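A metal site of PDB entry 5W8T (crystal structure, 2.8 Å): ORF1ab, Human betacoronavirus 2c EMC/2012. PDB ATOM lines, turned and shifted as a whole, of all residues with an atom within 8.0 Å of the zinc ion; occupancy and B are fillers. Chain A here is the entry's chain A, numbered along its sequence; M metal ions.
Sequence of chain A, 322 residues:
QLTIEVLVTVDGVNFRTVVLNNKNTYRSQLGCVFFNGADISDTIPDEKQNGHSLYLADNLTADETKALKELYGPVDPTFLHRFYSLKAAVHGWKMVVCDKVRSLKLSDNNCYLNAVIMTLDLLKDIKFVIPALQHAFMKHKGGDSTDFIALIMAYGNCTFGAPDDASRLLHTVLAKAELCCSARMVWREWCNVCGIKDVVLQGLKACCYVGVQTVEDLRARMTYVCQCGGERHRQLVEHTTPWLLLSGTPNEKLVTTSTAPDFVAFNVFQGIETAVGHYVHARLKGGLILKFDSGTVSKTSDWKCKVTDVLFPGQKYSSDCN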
ATOM      1  N   TRP A 190     -12.458   4.990 -16.828  1.00  0.00           N
ATOM      2  CA  TRP A 190     -12.092   6.389 -16.671  1.00  0.00           C
ATOM      3  C   TRP A 190     -13.293   7.289 -16.970  1.00  0.00           C
ATOM      4  O   TRP A 190     -14.247   6.879 -17.643  1.00  0.00           O
ATOM      5  CB  TRP A 190     -10.880   6.769 -17.539  1.00  0.00           C
ATOM      6  CG  TRP A 190     -11.070   6.719 -19.029  1.00  0.00           C
ATOM      7  CD1 TRP A 190     -11.390   7.762 -19.849  1.00  0.00           C
ATOM      8  CD2 TRP A 190     -10.917   5.572 -19.874  1.00  0.00           C
ATOM      9  NE1 TRP A 190     -11.457   7.331 -21.162  1.00  0.00           N
ATOM     10  CE2 TRP A 190     -11.175   5.995 -21.199  1.00  0.00           C
ATOM     11  CE3 TRP A 190     -10.602   4.236 -19.644  1.00  0.00           C
ATOM     12  CZ2 TRP A 190     -11.129   5.121 -22.282  1.00  0.00           C
ATOM     13  CZ3 TRP A 190     -10.551   3.370 -20.725  1.00  0.00           C
ATOM     14  CH2 TRP A 190     -10.809   3.812 -22.028  1.00  0.00           C
ATOM     15  N   CYS A 191     -13.248   8.492 -16.398  1.00  0.00           N
ATOM     16  CA  CYS A 191     -14.255   9.513 -16.598  1.00  0.00           C
ATOM     17  C   CYS A 191     -13.558  10.860 -16.536  1.00  0.00           C
ATOM     18  O   CYS A 191     -12.812  11.124 -15.590  1.00  0.00           O
ATOM     19  CB  CYS A 191     -15.351   9.432 -15.541  1.00  0.00           C
ATOM     20  SG  CYS A 191     -16.244  10.990 -15.273  1.00  0.00           S
ATOM     21  N   ASN A 192     -13.813  11.714 -17.540  1.00  0.00           N
ATOM     22  CA  ASN A 192     -13.118  12.993 -17.617  1.00  0.00           C
ATOM     23  C   ASN A 192     -13.287  13.841 -16.360  1.00  0.00           C
ATOM     24  O   ASN A 192     -12.476  14.741 -16.119  1.00  0.00           O
ATOM     25  CB  ASN A 192     -13.594  13.802 -18.837  1.00  0.00           C
ATOM     26  CG  ASN A 192     -13.187  13.163 -20.163  1.00  0.00           C
ATOM     27  OD1 ASN A 192     -12.408  12.214 -20.196  1.00  0.00           O
ATOM     28  ND2 ASN A 192     -13.710  13.713 -21.255  1.00  0.00           N
ATOM     29  N   VAL A 193     -14.295  13.566 -15.536  1.00  0.00           N
ATOM     30  CA  VAL A 193     -14.540  14.315 -14.320  1.00  0.00           C
ATOM     31  C   VAL A 193     -14.092  13.555 -13.077  1.00  0.00           C
ATOM     32  O   VAL A 193     -13.565  14.157 -12.144  1.00  0.00           O
ATOM     33  CB  VAL A 193     -16.037  14.692 -14.227  1.00  0.00           C
ATOM     34  CG1 VAL A 193     -16.289  15.693 -13.106  1.00  0.00           C
ATOM     35  CG2 VAL A 193     -16.517  15.269 -15.544  1.00  0.00           C
ATOM     36  N   CYS A 194     -14.259  12.234 -13.059  1.00  0.00           N
ATOM     37  CA  CYS A 194     -14.006  11.430 -11.867  1.00  0.00           C
ATOM     38  C   CYS A 194     -12.587  10.898 -11.774  1.00  0.00           C
ATOM     39  O   CYS A 194     -12.008  10.868 -10.679  1.00  0.00           O
ATOM     40  CB  CYS A 194     -14.980  10.254 -11.815  1.00  0.00           C
ATOM     41  SG  CYS A 194     -16.695  10.744 -11.636  1.00  0.00           S
ATOM     42  N   GLY A 195     -11.989  10.455 -12.881  1.00  0.00           N
ATOM     43  CA  GLY A 195     -10.623   9.982 -12.849  1.00  0.00           C
ATOM     44  C   GLY A 195     -10.492   8.637 -13.526  1.00  0.00           C
ATOM     45  O   GLY A 195     -11.388   8.201 -14.265  1.00  0.00           O
ATOM     46  N   TYR A 224     -20.798   4.254 -21.097  1.00  0.00           N
ATOM     47  CA  TYR A 224     -22.061   4.203 -20.382  1.00  0.00           C
ATOM     48  C   TYR A 224     -22.099   5.355 -19.390  1.00  0.00           C
ATOM     49  O   TYR A 224     -21.105   6.057 -19.176  1.00  0.00           O
ATOM     50  CB  TYR A 224     -22.261   2.855 -19.671  1.00  0.00           C
ATOM     51  CG  TYR A 224     -21.082   2.442 -18.815  1.00  0.00           C
ATOM     52  CD1 TYR A 224     -19.941   1.868 -19.380  1.00  0.00           C
ATOM     53  CD2 TYR A 224     -21.105   2.615 -17.430  1.00  0.00           C
ATOM     54  CE1 TYR A 224     -18.867   1.490 -18.594  1.00  0.00           C
ATOM     55  CE2 TYR A 224     -20.031   2.237 -16.644  1.00  0.00           C
ATOM     56  CZ  TYR A 224     -18.913   1.681 -17.231  1.00  0.00           C
ATOM     57  OH  TYR A 224     -17.839   1.302 -16.445  1.00  0.00           O
ATOM     58  N   VAL A 225     -23.268   5.563 -18.776  1.00  0.00           N
ATOM     59  CA  VAL A 225     -23.434   6.743 -17.929  1.00  0.00           C
ATOM     60  C   VAL A 225     -22.652   6.565 -16.632  1.00  0.00           C
ATOM     61  O   VAL A 225     -22.650   5.479 -16.019  1.00  0.00           O
ATOM     62  CB  VAL A 225     -24.918   7.028 -17.652  1.00  0.00           C
ATOM     63  CG1 VAL A 225     -25.534   5.995 -16.727  1.00  0.00           C
ATOM     64  CG2 VAL A 225     -25.073   8.436 -17.094  1.00  0.00           C
ATOM     65  N   CYS A 226     -21.977   7.619 -16.229  1.00  0.00           N
ATOM     66  CA  CYS A 226     -21.181   7.638 -14.999  1.00  0.00           C
ATOM     67  C   CYS A 226     -22.031   8.139 -13.837  1.00  0.00           C
ATOM     68  O   CYS A 226     -23.104   8.715 -14.013  1.00  0.00           O
ATOM     69  CB  CYS A 226     -19.952   8.517 -15.183  1.00  0.00           C
ATOM     70  SG  CYS A 226     -18.751   8.468 -13.839  1.00  0.00           S
ATOM     71  N   GLN A 227     -21.538   7.898 -12.614  1.00  0.00           N
ATOM     72  CA  GLN A 227     -22.309   8.284 -11.444  1.00  0.00           C
ATOM     73  C   GLN A 227     -22.393   9.800 -11.310  1.00  0.00           C
ATOM     74  O   GLN A 227     -23.270  10.296 -10.598  1.00  0.00           O
ATOM     75  CB  GLN A 227     -21.700   7.659 -10.187  1.00  0.00           C
ATOM     76  CG  GLN A 227     -22.628   7.756  -8.987  1.00  0.00           C
ATOM     77  CD  GLN A 227     -21.997   7.278  -7.690  1.00  0.00           C
ATOM     78  OE1 GLN A 227     -20.930   6.657  -7.702  1.00  0.00           O
ATOM     79  NE2 GLN A 227     -22.646   7.571  -6.575  1.00  0.00           N
ATOM     80  N   CYS A 228     -21.511  10.530 -12.001  1.00  0.00           N
ATOM     81  CA  CYS A 228     -21.507  11.984 -12.025  1.00  0.00           C
ATOM     82  C   CYS A 228     -22.508  12.563 -13.033  1.00  0.00           C
ATOM     83  O   CYS A 228     -22.895  13.731 -12.895  1.00  0.00           O
ATOM     84  CB  CYS A 228     -20.099  12.486 -12.369  1.00  0.00           C
ATOM     85  SG  CYS A 228     -19.595  12.195 -14.080  1.00  0.00           S
ATOM     86  N   GLY A 229     -22.930  11.770 -14.025  1.00  0.00           N
ATOM     87  CA  GLY A 229     -23.803  12.229 -15.091  1.00  0.00           C
ATOM     88  C   GLY A 229     -23.161  12.230 -16.458  1.00  0.00           C
ATOM     89  O   GLY A 229     -23.868  12.147 -17.470  1.00  0.00           O
ATOM     90  N   GLY A 230     -21.828  12.316 -16.522  1.00  0.00           N
ATOM     91  CA  GLY A 230     -21.093  12.233 -17.765  1.00  0.00           C
ATOM     92  C   GLY A 230     -21.095  10.821 -18.334  1.00  0.00           C
ATOM     93  O   GLY A 230     -21.845   9.944 -17.897  1.00  0.00           O
ATOM     94  N   GLU A 231     -20.226  10.600 -19.322  1.00  0.00           N
ATOM     95  CA  GLU A 231     -20.063   9.258 -19.872  1.00  0.00           C
ATOM     96  C   GLU A 231     -18.747   8.658 -19.384  1.00  0.00           C
ATOM     97  O   GLU A 231     -17.668   9.193 -19.665  1.00  0.00           O
ATOM     98  CB  GLU A 231     -20.164   9.194 -21.403  1.00  0.00           C
ATOM     99  CG  GLU A 231     -19.812  10.401 -22.211  1.00  0.00           C
ATOM    100  CD  GLU A 231     -20.063  10.149 -23.700  1.00  0.00           C
ATOM    101  OE1 GLU A 231     -20.688   9.138 -24.062  1.00  0.00           O
ATOM    102  OE2 GLU A 231     -19.684  10.978 -24.525  1.00  0.00           O
ATOM    103  N   ARG A 232     -18.861   7.571 -18.624  1.00  0.00           N
ATOM    104  CA  ARG A 232     -17.719   6.794 -18.197  1.00  0.00           C
ATOM    105  C   ARG A 232     -17.314   5.824 -19.305  1.00  0.00           C
ATOM    106  O   ARG A 232     -18.157   5.321 -20.066  1.00  0.00           O
ATOM    107  CB  ARG A 232     -18.044   6.032 -16.902  1.00  0.00           C
ATOM    108  CG  ARG A 232     -16.909   5.203 -16.309  1.00  0.00           C
ATOM    109  CD  ARG A 232     -17.176   4.832 -14.853  1.00  0.00           C
ATOM    110  NE  ARG A 232     -18.567   4.417 -14.639  1.00  0.00           N
ATOM    111  CZ  ARG A 232     -19.050   3.910 -13.509  1.00  0.00           C
ATOM    112  NH1 ARG A 232     -18.262   3.739 -12.453  1.00  0.00           N
ATOM    113  NH2 ARG A 232     -20.328   3.566 -13.425  1.00  0.00           N
ATOM    114  N   HIS A 233     -16.017   5.563 -19.391  1.00  0.00           N
ATOM    115  CA  HIS A 233     -15.482   4.639 -20.365  1.00  0.00           C
ATOM    116  C   HIS A 233     -14.855   3.452 -19.643  1.00  0.00           C
ATOM    117  O   HIS A 233     -14.444   3.555 -18.485  1.00  0.00           O
ATOM    118  CB  HIS A 233     -14.475   5.341 -21.266  1.00  0.00           C
ATOM    119  CG  HIS A 233     -15.051   6.530 -21.981  1.00  0.00           C
ATOM    120  ND1 HIS A 233     -15.866   6.403 -23.093  1.00  0.00           N
ATOM    121  CD2 HIS A 233     -14.946   7.853 -21.733  1.00  0.00           C
ATOM    122  CE1 HIS A 233     -16.231   7.613 -23.495  1.00  0.00           C
ATOM    123  NE2 HIS A 233     -15.684   8.506 -22.700  1.00  0.00           N
HETATM  124 ZN    ZN M   1     -17.988  10.701 -13.702  1.00  0.00          ZN
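The side-chain sulfur (SG) of Cys 228 lies close to the backbone NH (N) of Gly 230, at 3.3 Å. SG of Cys 191 sits close to N of Val 193, 3.2 Å away.
Of the 16 residues printed, 4 come within 4 Å of the zinc ion. The nearest printed residue that does not touch the zinc ion is Val 193 (4.5 Å).
The zinc ion is bound by the side-chain sulfur (SG) of Cys 228 (2.2 Å), the side-chain sulfur (SG) of Cys 226 (2.4 Å), the side-chain sulfur (SG) of Cys 191 (2.4 Å) and the side-chain sulfur (SG) of Cys 194 (2.4 Å).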
